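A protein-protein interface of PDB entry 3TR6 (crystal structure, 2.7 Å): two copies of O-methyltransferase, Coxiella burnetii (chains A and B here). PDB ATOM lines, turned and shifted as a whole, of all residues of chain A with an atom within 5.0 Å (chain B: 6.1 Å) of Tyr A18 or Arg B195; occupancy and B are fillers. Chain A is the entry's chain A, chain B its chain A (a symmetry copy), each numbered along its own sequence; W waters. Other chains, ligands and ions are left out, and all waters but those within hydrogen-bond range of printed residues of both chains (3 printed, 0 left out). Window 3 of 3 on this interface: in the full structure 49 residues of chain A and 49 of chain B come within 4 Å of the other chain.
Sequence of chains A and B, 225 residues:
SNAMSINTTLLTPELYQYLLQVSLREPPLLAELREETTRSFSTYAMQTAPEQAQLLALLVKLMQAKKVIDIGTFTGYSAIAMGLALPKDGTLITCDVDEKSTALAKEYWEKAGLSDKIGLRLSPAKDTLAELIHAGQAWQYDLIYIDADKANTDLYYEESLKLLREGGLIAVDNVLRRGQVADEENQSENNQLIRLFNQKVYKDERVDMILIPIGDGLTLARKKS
Water W3 lies within hydrogen-bond range of the side-chain hydroxyl of Tyr A18 (2.5 Å) and the backbone carbonyl oxygen of Arg B195 (2.8 Å). Water W2 lies within hydrogen-bond range of O of Asn B198 (2.7 Å) and O of Val A22 (2.9 Å). Water W1 lies within hydrogen-bond range of OE1 of Gln A21 (2.8 Å) and NE2 of Gln B199 (3.1 Å).
The side-chain hydroxyl of Tyr A18 sits at hydrogen-bond distance from the side-chain amide nitrogen of Asn B198, 2.9 Å away.
No position is printed for both chains.
Hydrophobic or aromatic side chains of chain A that line the printed part of chain B: Leu A15, Tyr A18, Leu A19 and Val A22. Of the 19 printed residues of chain B, 6 touch a printed residue of chain A. Hydrophobic or aromatic side chains of chain B that line the printed part of chain A: Val B181, Ala B182 and Leu B211. Among the printed residues, no Asp or Glu carboxylate lies within 4 Å of a Lys or Arg side-chain nitrogen of the other chain.
Tyr A18 touches just these residues of chain B: Val B181, Ala B182, Arg B195 and Asn B198. Of the printed residues of chain A, Arg B195 touches Tyr A18. Of the printed residues of chain A, Gln B199 touches Val A22 (3.5 Å). Printed residues of chain A within 4 Å of Ala B182: Leu A15 and Tyr A18. Of the printed residues of chain A, Asn B198 touches Tyr A18. Gln A17 touches none of the printed residues of chain B. Phe B197 touches none of the printed residues of chain A. The nearest residue of chain B that does not touch Tyr A18 is Leu B176 (4.4 Å). The nearest printed residue of chain A that does not touch Arg B195 is Val A22 (5.7 Å). The nearest printed residue of chain B that does not touch Leu A19 is Leu B176 (4.8 Å).
Among the printed residues, merely in contact across the chains: Tyr A18 with Val B181, Val A22 with Gln B199, Leu A19 with Leu B211, Val A22 with Leu B211, Tyr A18 with Arg B195, Tyr A18 with Ala B182 and Leu A15 with Ala B182.
NH2 of Arg B195 is in salt-bridge range of OE1 of Glu B184, 3.7 Å away. The side-chain amide oxygen of Asn B191 is in hydrogen-bond range of the backbone NH of Val B181 (3.5 Å). The backbone carbonyl oxygen (O) of Val B181 sits at hydrogen-bond distance from the guanidinium group (NH1) of Arg B195, at 2.8 Å. ND2 of Asn B198 lies within hydrogen-bond range of O of Val B175, 3.0 Å away. The backbone carbonyl oxygen (O) of Ile B194 sits close to the side-chain amide nitrogen (ND2) of Asn B198 (3.3 Å).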
ATOM      1  N   GLU A  14     -19.880 -28.223  -6.197  1.00  0.00           N
ATOM      2  CA  GLU A  14     -18.663 -27.505  -5.838  1.00  0.00           C
ATOM      3  C   GLU A  14     -17.855 -28.286  -4.808  1.00  0.00           C
ATOM      4  O   GLU A  14     -16.678 -28.580  -5.015  1.00  0.00           O
ATOM      5  CB  GLU A  14     -18.994 -26.114  -5.290  1.00  0.00           C
ATOM      6  CG  GLU A  14     -19.495 -25.120  -6.337  1.00  0.00           C
ATOM      7  CD  GLU A  14     -20.885 -25.457  -6.873  1.00  0.00           C
ATOM      8  OE1 GLU A  14     -21.751 -25.893  -6.080  1.00  0.00           O
ATOM      9  OE2 GLU A  14     -21.111 -25.286  -8.092  1.00  0.00           O
ATOM     10  N   LEU A  15     -18.502 -28.620  -3.698  1.00  0.00           N
ATOM     11  CA  LEU A  15     -17.845 -29.334  -2.615  1.00  0.00           C
ATOM     12  C   LEU A  15     -17.391 -30.721  -3.068  1.00  0.00           C
ATOM     13  O   LEU A  15     -16.302 -31.172  -2.715  1.00  0.00           O
ATOM     14  CB  LEU A  15     -18.775 -29.434  -1.405  1.00  0.00           C
ATOM     15  CG  LEU A  15     -18.136 -29.833  -0.076  1.00  0.00           C
ATOM     16  CD1 LEU A  15     -16.953 -28.934   0.242  1.00  0.00           C
ATOM     17  CD2 LEU A  15     -19.162 -29.798   1.047  1.00  0.00           C
ATOM     18  N   TYR A  16     -18.227 -31.391  -3.856  1.00  0.00           N
ATOM     19  CA  TYR A  16     -17.883 -32.705  -4.387  1.00  0.00           C
ATOM     20  C   TYR A  16     -16.565 -32.673  -5.157  1.00  0.00           C
ATOM     21  O   TYR A  16     -15.705 -33.533  -4.969  1.00  0.00           O
ATOM     22  CB  TYR A  16     -19.001 -33.246  -5.282  1.00  0.00           C
ATOM     23  CG  TYR A  16     -18.604 -34.475  -6.076  1.00  0.00           C
ATOM     24  CD1 TYR A  16     -18.520 -35.725  -5.471  1.00  0.00           C
ATOM     25  CD2 TYR A  16     -18.315 -34.385  -7.432  1.00  0.00           C
ATOM     26  CE1 TYR A  16     -18.156 -36.848  -6.195  1.00  0.00           C
ATOM     27  CE2 TYR A  16     -17.951 -35.500  -8.162  1.00  0.00           C
ATOM     28  CZ  TYR A  16     -17.874 -36.729  -7.542  1.00  0.00           C
ATOM     29  OH  TYR A  16     -17.511 -37.839  -8.270  1.00  0.00           O
ATOM     30  N   GLN A  17     -16.410 -31.677  -6.022  1.00  0.00           N
ATOM     31  CA  GLN A  17     -15.195 -31.553  -6.816  1.00  0.00           C
ATOM     32  C   GLN A  17     -13.982 -31.297  -5.936  1.00  0.00           C
ATOM     33  O   GLN A  17     -12.899 -31.826  -6.187  1.00  0.00           O
ATOM     34  CB  GLN A  17     -15.340 -30.444  -7.860  1.00  0.00           C
ATOM     35  CG  GLN A  17     -16.274 -30.804  -9.003  1.00  0.00           C
ATOM     36  CD  GLN A  17     -15.815 -32.032  -9.763  1.00  0.00           C
ATOM     37  OE1 GLN A  17     -14.630 -32.373  -9.753  1.00  0.00           O
ATOM     38  NE2 GLN A  17     -16.749 -32.708 -10.421  1.00  0.00           N
ATOM     39  N   TYR A  18     -14.165 -30.476  -4.907  1.00  0.00           N
ATOM     40  CA  TYR A  18     -13.087 -30.198  -3.971  1.00  0.00           C
ATOM     41  C   TYR A  18     -12.672 -31.476  -3.257  1.00  0.00           C
ATOM     42  O   TYR A  18     -11.489 -31.716  -3.026  1.00  0.00           O
ATOM     43  CB  TYR A  18     -13.501 -29.135  -2.950  1.00  0.00           C
ATOM     44  CG  TYR A  18     -12.515 -29.017  -1.817  1.00  0.00           C
ATOM     45  CD1 TYR A  18     -11.358 -28.269  -1.962  1.00  0.00           C
ATOM     46  CD2 TYR A  18     -12.724 -29.681  -0.612  1.00  0.00           C
ATOM     47  CE1 TYR A  18     -10.443 -28.173  -0.943  1.00  0.00           C
ATOM     48  CE2 TYR A  18     -11.809 -29.590   0.417  1.00  0.00           C
ATOM     49  CZ  TYR A  18     -10.669 -28.833   0.244  1.00  0.00           C
ATOM     50  OH  TYR A  18      -9.740 -28.720   1.252  1.00  0.00           O
ATOM     51  N   LEU A  19     -13.657 -32.295  -2.907  1.00  0.00           N
ATOM     52  CA  LEU A  19     -13.398 -33.549  -2.210  1.00  0.00           C
ATOM     53  C   LEU A  19     -12.503 -34.458  -3.044  1.00  0.00           C
ATOM     54  O   LEU A  19     -11.533 -35.023  -2.537  1.00  0.00           O
ATOM     55  CB  LEU A  19     -14.714 -34.250  -1.864  1.00  0.00           C
ATOM     56  CG  LEU A  19     -14.650 -35.567  -1.093  1.00  0.00           C
ATOM     57  CD1 LEU A  19     -15.915 -35.762  -0.279  1.00  0.00           C
ATOM     58  CD2 LEU A  19     -14.425 -36.746  -2.033  1.00  0.00           C
ATOM     59  N   LEU A  20     -12.824 -34.593  -4.326  1.00  0.00           N
ATOM     60  CA  LEU A  20     -12.010 -35.399  -5.225  1.00  0.00           C
ATOM     61  C   LEU A  20     -10.587 -34.851  -5.315  1.00  0.00           C
ATOM     62  O   LEU A  20      -9.625 -35.612  -5.419  1.00  0.00           O
ATOM     63  CB  LEU A  20     -12.633 -35.471  -6.619  1.00  0.00           C
ATOM     64  CG  LEU A  20     -14.012 -36.114  -6.741  1.00  0.00           C
ATOM     65  CD1 LEU A  20     -14.470 -36.098  -8.194  1.00  0.00           C
ATOM     66  CD2 LEU A  20     -14.002 -37.532  -6.197  1.00  0.00           C
ATOM     67  N   GLN A  21     -10.458 -33.530  -5.267  1.00  0.00           N
ATOM     68  CA  GLN A  21      -9.154 -32.890  -5.396  1.00  0.00           C
ATOM     69  C   GLN A  21      -8.245 -33.158  -4.205  1.00  0.00           C
ATOM     70  O   GLN A  21      -7.024 -33.107  -4.329  1.00  0.00           O
ATOM     71  CB  GLN A  21      -9.313 -31.384  -5.604  1.00  0.00           C
ATOM     72  CG  GLN A  21      -9.947 -31.015  -6.938  1.00  0.00           C
ATOM     73  CD  GLN A  21     -10.315 -29.545  -7.028  1.00  0.00           C
ATOM     74  OE1 GLN A  21     -10.022 -28.762  -6.122  1.00  0.00           O
ATOM     75  NE2 GLN A  21     -10.965 -29.164  -8.124  1.00  0.00           N
ATOM     76  N   VAL A  22      -8.840 -33.437  -3.050  1.00  0.00           N
ATOM     77  CA  VAL A  22      -8.059 -33.674  -1.843  1.00  0.00           C
ATOM     78  C   VAL A  22      -8.159 -35.105  -1.331  1.00  0.00           C
ATOM     79  O   VAL A  22      -7.735 -35.391  -0.212  1.00  0.00           O
ATOM     80  CB  VAL A  22      -8.448 -32.706  -0.703  1.00  0.00           C
ATOM     81  CG1 VAL A  22      -8.130 -31.278  -1.095  1.00  0.00           C
ATOM     82  CG2 VAL A  22      -9.922 -32.867  -0.336  1.00  0.00           C
ATOM     83  N   VAL B 175     -13.172 -31.762   8.203  1.00  0.00           N
ATOM     84  CA  VAL B 175     -12.263 -31.421   7.111  1.00  0.00           C
ATOM     85  C   VAL B 175     -12.957 -30.648   5.988  1.00  0.00           C
ATOM     86  O   VAL B 175     -12.297 -30.105   5.106  1.00  0.00           O
ATOM     87  CB  VAL B 175     -11.575 -32.675   6.522  1.00  0.00           C
ATOM     88  CG1 VAL B 175     -10.523 -33.205   7.482  1.00  0.00           C
ATOM     89  CG2 VAL B 175     -12.606 -33.746   6.187  1.00  0.00           C
ATOM     90  N   LEU B 176     -14.287 -30.596   6.022  1.00  0.00           N
ATOM     91  CA  LEU B 176     -15.041 -29.894   4.985  1.00  0.00           C
ATOM     92  C   LEU B 176     -15.495 -28.505   5.430  1.00  0.00           C
ATOM     93  O   LEU B 176     -15.794 -27.647   4.598  1.00  0.00           O
ATOM     94  CB  LEU B 176     -16.239 -30.723   4.508  1.00  0.00           C
ATOM     95  CG  LEU B 176     -15.890 -32.001   3.743  1.00  0.00           C
ATOM     96  CD1 LEU B 176     -17.145 -32.722   3.262  1.00  0.00           C
ATOM     97  CD2 LEU B 176     -14.960 -31.697   2.576  1.00  0.00           C
ATOM     98  N   GLN B 180     -17.091 -24.294   3.592  1.00  0.00           N
ATOM     99  CA  GLN B 180     -16.197 -23.139   3.514  1.00  0.00           C
ATOM    100  C   GLN B 180     -14.857 -23.483   2.884  1.00  0.00           C
ATOM    101  O   GLN B 180     -14.179 -22.622   2.324  1.00  0.00           O
ATOM    102  CB  GLN B 180     -15.935 -22.570   4.906  1.00  0.00           C
ATOM    103  CG  GLN B 180     -17.121 -21.912   5.569  1.00  0.00           C
ATOM    104  CD  GLN B 180     -16.747 -21.290   6.899  1.00  0.00           C
ATOM    105  OE1 GLN B 180     -15.817 -20.483   6.981  1.00  0.00           O
ATOM    106  NE2 GLN B 180     -17.458 -21.676   7.954  1.00  0.00           N
ATOM    107  N   VAL B 181     -14.475 -24.748   2.994  1.00  0.00           N
ATOM    108  CA  VAL B 181     -13.145 -25.186   2.605  1.00  0.00           C
ATOM    109  C   VAL B 181     -12.964 -25.141   1.086  1.00  0.00           C
ATOM    110  O   VAL B 181     -11.846 -25.038   0.586  1.00  0.00           O
ATOM    111  CB  VAL B 181     -12.851 -26.599   3.170  1.00  0.00           C
ATOM    112  CG1 VAL B 181     -13.581 -27.663   2.363  1.00  0.00           C
ATOM    113  CG2 VAL B 181     -11.359 -26.868   3.209  1.00  0.00           C
ATOM    114  N   ALA B 182     -14.075 -25.197   0.360  1.00  0.00           N
ATOM    115  CA  ALA B 182     -14.044 -25.153  -1.098  1.00  0.00           C
ATOM    116  C   ALA B 182     -13.979 -23.717  -1.607  1.00  0.00           C
ATOM    117  O   ALA B 182     -13.701 -23.477  -2.782  1.00  0.00           O
ATOM    118  CB  ALA B 182     -15.250 -25.870  -1.679  1.00  0.00           C
ATOM    119  N   ASP B 183     -14.243 -22.766  -0.715  1.00  0.00           N
ATOM    120  CA  ASP B 183     -14.170 -21.348  -1.051  1.00  0.00           C
ATOM    121  C   ASP B 183     -12.768 -20.811  -0.786  1.00  0.00           C
ATOM    122  O   ASP B 183     -12.458 -20.377   0.325  1.00  0.00           O
ATOM    123  CB  ASP B 183     -15.202 -20.556  -0.248  1.00  0.00           C
ATOM    124  CG  ASP B 183     -15.187 -19.079  -0.579  1.00  0.00           C
ATOM    125  OD1 ASP B 183     -14.713 -18.713  -1.677  1.00  0.00           O
ATOM    126  OD2 ASP B 183     -15.656 -18.281   0.259  1.00  0.00           O
ATOM    127  N   GLU B 184     -11.929 -20.843  -1.816  1.00  0.00           N
ATOM    128  CA  GLU B 184     -10.527 -20.453  -1.695  1.00  0.00           C
ATOM    129  C   GLU B 184     -10.352 -19.030  -1.163  1.00  0.00           C
ATOM    130  O   GLU B 184      -9.273 -18.657  -0.696  1.00  0.00           O
ATOM    131  CB  GLU B 184      -9.826 -20.593  -3.049  1.00  0.00           C
ATOM    132  CG  GLU B 184      -8.320 -20.393  -3.000  1.00  0.00           C
ATOM    133  CD  GLU B 184      -7.689 -20.389  -4.380  1.00  0.00           C
ATOM    134  OE1 GLU B 184      -6.982 -21.363  -4.719  1.00  0.00           O
ATOM    135  OE2 GLU B 184      -7.902 -19.410  -5.126  1.00  0.00           O
ATOM    136  N   ASN B 190      -8.641 -20.273  10.379  1.00  0.00           N
ATOM    137  CA  ASN B 190      -8.881 -21.706  10.487  1.00  0.00           C
ATOM    138  C   ASN B 190      -9.175 -22.382   9.151  1.00  0.00           C
ATOM    139  O   ASN B 190      -8.831 -23.546   8.944  1.00  0.00           O
ATOM    140  CB  ASN B 190      -9.997 -21.995  11.493  1.00  0.00           C
ATOM    141  CG  ASN B 190      -9.469 -22.544  12.805  1.00  0.00           C
ATOM    142  OD1 ASN B 190      -8.258 -22.589  13.029  1.00  0.00           O
ATOM    143  ND2 ASN B 190     -10.376 -22.965  13.679  1.00  0.00           N
ATOM    144  N   ASN B 191      -9.810 -21.652   8.243  1.00  0.00           N
ATOM    145  CA  ASN B 191     -10.131 -22.214   6.939  1.00  0.00           C
ATOM    146  C   ASN B 191      -8.875 -22.468   6.111  1.00  0.00           C
ATOM    147  O   ASN B 191      -8.771 -23.482   5.426  1.00  0.00           O
ATOM    148  CB  ASN B 191     -11.102 -21.311   6.181  1.00  0.00           C
ATOM    149  CG  ASN B 191     -11.784 -22.027   5.039  1.00  0.00           C
ATOM    150  OD1 ASN B 191     -12.673 -22.851   5.257  1.00  0.00           O
ATOM    151  ND2 ASN B 191     -11.376 -21.717   3.815  1.00  0.00           N
ATOM    152  N   GLN B 192      -7.920 -21.549   6.185  1.00  0.00           N
ATOM    153  CA  GLN B 192      -6.660 -21.713   5.471  1.00  0.00           C
ATOM    154  C   GLN B 192      -5.821 -22.855   6.050  1.00  0.00           C
ATOM    155  O   GLN B 192      -5.092 -23.528   5.322  1.00  0.00           O
ATOM    156  CB  GLN B 192      -5.867 -20.403   5.469  1.00  0.00           C
ATOM    157  CG  GLN B 192      -6.376 -19.371   4.469  1.00  0.00           C
ATOM    158  CD  GLN B 192      -6.140 -19.787   3.024  1.00  0.00           C
ATOM    159  OE1 GLN B 192      -7.082 -20.079   2.283  1.00  0.00           O
ATOM    160  NE2 GLN B 192      -4.875 -19.807   2.613  1.00  0.00           N
ATOM    161  N   LEU B 193      -5.932 -23.071   7.358  1.00  0.00           N
ATOM    162  CA  LEU B 193      -5.221 -24.167   8.011  1.00  0.00           C
ATOM    163  C   LEU B 193      -5.723 -25.530   7.545  1.00  0.00           C
ATOM    164  O   LEU B 193      -4.932 -26.450   7.334  1.00  0.00           O
ATOM    165  CB  LEU B 193      -5.336 -24.072   9.535  1.00  0.00           C
ATOM    166  CG  LEU B 193      -4.310 -23.194  10.247  1.00  0.00           C
ATOM    167  CD1 LEU B 193      -4.362 -23.447  11.740  1.00  0.00           C
ATOM    168  CD2 LEU B 193      -2.912 -23.462   9.709  1.00  0.00           C
ATOM    169  N   ILE B 194      -7.039 -25.653   7.395  1.00  0.00           N
ATOM    170  CA  ILE B 194      -7.651 -26.914   6.993  1.00  0.00           C
ATOM    171  C   ILE B 194      -7.461 -27.179   5.504  1.00  0.00           C
ATOM    172  O   ILE B 194      -7.295 -28.324   5.086  1.00  0.00           O
ATOM    173  CB  ILE B 194      -9.146 -26.964   7.359  1.00  0.00           C
ATOM    174  CG1 ILE B 194      -9.312 -26.928   8.877  1.00  0.00           C
ATOM    175  CG2 ILE B 194      -9.796 -28.214   6.791  1.00  0.00           C
ATOM    176  CD1 ILE B 194      -8.405 -27.904   9.605  1.00  0.00           C
ATOM    177  N   ARG B 195      -7.483 -26.119   4.702  1.00  0.00           N
ATOM    178  CA  ARG B 195      -7.198 -26.255   3.280  1.00  0.00           C
ATOM    179  C   ARG B 195      -5.758 -26.713   3.093  1.00  0.00           C
ATOM    180  O   ARG B 195      -5.469 -27.588   2.277  1.00  0.00           O
ATOM    181  CB  ARG B 195      -7.453 -24.940   2.538  1.00  0.00           C
ATOM    182  CG  ARG B 195      -8.924 -24.669   2.256  1.00  0.00           C
ATOM    183  CD  ARG B 195      -9.122 -23.365   1.498  1.00  0.00           C
ATOM    184  NE  ARG B 195      -8.230 -23.269   0.347  1.00  0.00           N
ATOM    185  CZ  ARG B 195      -8.507 -23.749  -0.862  1.00  0.00           C
ATOM    186  NH1 ARG B 195      -9.662 -24.362  -1.088  1.00  0.00           N
ATOM    187  NH2 ARG B 195      -7.628 -23.614  -1.847  1.00  0.00           N
ATOM    188  N   LEU B 196      -4.856 -26.124   3.869  1.00  0.00           N
ATOM    189  CA  LEU B 196      -3.452 -26.500   3.826  1.00  0.00           C
ATOM    190  C   LEU B 196      -3.276 -27.940   4.301  1.00  0.00           C
ATOM    191  O   LEU B 196      -2.460 -28.684   3.758  1.00  0.00           O
ATOM    192  CB  LEU B 196      -2.624 -25.551   4.694  1.00  0.00           C
ATOM    193  CG  LEU B 196      -1.104 -25.639   4.545  1.00  0.00           C
ATOM    194  CD1 LEU B 196      -0.687 -25.277   3.126  1.00  0.00           C
ATOM    195  CD2 LEU B 196      -0.414 -24.740   5.559  1.00  0.00           C
ATOM    196  N   PHE B 197      -4.050 -28.323   5.313  1.00  0.00           N
ATOM    197  CA  PHE B 197      -3.961 -29.656   5.904  1.00  0.00           C
ATOM    198  C   PHE B 197      -4.470 -30.751   4.970  1.00  0.00           C
ATOM    199  O   PHE B 197      -3.847 -31.807   4.842  1.00  0.00           O
ATOM    200  CB  PHE B 197      -4.728 -29.709   7.232  1.00  0.00           C
ATOM    201  CG  PHE B 197      -4.843 -31.091   7.812  1.00  0.00           C
ATOM    202  CD1 PHE B 197      -3.825 -31.625   8.589  1.00  0.00           C
ATOM    203  CD2 PHE B 197      -5.973 -31.861   7.581  1.00  0.00           C
ATOM    204  CE1 PHE B 197      -3.932 -32.902   9.123  1.00  0.00           C
ATOM    205  CE2 PHE B 197      -6.086 -33.137   8.112  1.00  0.00           C
ATOM    206  CZ  PHE B 197      -5.066 -33.657   8.883  1.00  0.00           C
ATOM    207  N   ASN B 198      -5.605 -30.497   4.326  1.00  0.00           N
ATOM    208  CA  ASN B 198      -6.193 -31.463   3.407  1.00  0.00           C
ATOM    209  C   ASN B 198      -5.267 -31.810   2.249  1.00  0.00           C
ATOM    210  O   ASN B 198      -5.194 -32.962   1.831  1.00  0.00           O
ATOM    211  CB  ASN B 198      -7.541 -30.966   2.881  1.00  0.00           C
ATOM    212  CG  ASN B 198      -8.624 -30.978   3.942  1.00  0.00           C
ATOM    213  OD1 ASN B 198      -8.544 -31.718   4.921  1.00  0.00           O
ATOM    214  ND2 ASN B 198      -9.649 -30.157   3.748  1.00  0.00           N
ATOM    215  N   GLN B 199      -4.562 -30.807   1.732  1.00  0.00           N
ATOM    216  CA  GLN B 199      -3.594 -31.026   0.660  1.00  0.00           C
ATOM    217  C   GLN B 199      -2.388 -31.804   1.171  1.00  0.00           C
ATOM    218  O   GLN B 199      -1.847 -32.659   0.470  1.00  0.00           O
ATOM    219  CB  GLN B 199      -3.144 -29.699   0.049  1.00  0.00           C
ATOM    220  CG  GLN B 199      -4.217 -28.997  -0.769  1.00  0.00           C
ATOM    221  CD  GLN B 199      -4.572 -29.747  -2.051  1.00  0.00           C
ATOM    222  OE1 GLN B 199      -3.851 -30.654  -2.477  1.00  0.00           O
ATOM    223  NE2 GLN B 199      -5.690 -29.365  -2.672  1.00  0.00           N
ATOM    224  N   LYS B 200      -1.972 -31.501   2.393  1.00  0.00           N
ATOM    225  CA  LYS B 200      -0.855 -32.191   3.022  1.00  0.00           C
ATOM    226  C   LYS B 200      -1.129 -33.693   3.145  1.00  0.00           C
ATOM    227  O   LYS B 200      -0.284 -34.516   2.782  1.00  0.00           O
ATOM    228  CB  LYS B 200      -0.559 -31.578   4.394  1.00  0.00           C
ATOM    229  CG  LYS B 200       0.617 -32.194   5.127  1.00  0.00           C
ATOM    230  CD  LYS B 200       0.157 -33.199   6.169  1.00  0.00           C
ATOM    231  CE  LYS B 200       1.285 -33.551   7.125  1.00  0.00           C
ATOM    232  NZ  LYS B 200       1.788 -32.352   7.857  1.00  0.00           N
ATOM    233  N   LEU B 211     -11.611 -39.519   1.966  1.00  0.00           N
ATOM    234  CA  LEU B 211     -12.406 -38.493   2.630  1.00  0.00           C
ATOM    235  C   LEU B 211     -13.895 -38.814   2.506  1.00  0.00           C
ATOM    236  O   LEU B 211     -14.479 -38.698   1.426  1.00  0.00           O
ATOM    237  CB  LEU B 211     -12.099 -37.112   2.053  1.00  0.00           C
ATOM    238  CG  LEU B 211     -12.473 -35.896   2.905  1.00  0.00           C
ATOM    239  CD1 LEU B 211     -11.817 -34.642   2.345  1.00  0.00           C
ATOM    240  CD2 LEU B 211     -13.984 -35.717   3.006  1.00  0.00           C
HETATM  241  O   HOH W   1      -7.923 -28.095  -4.429  1.00  0.00           O
HETATM  242  O   HOH W   2      -7.119 -34.701   2.580  1.00  0.00           O
HETATM  243  O   HOH W   3      -7.538 -27.768   0.438  1.00  0.00           O
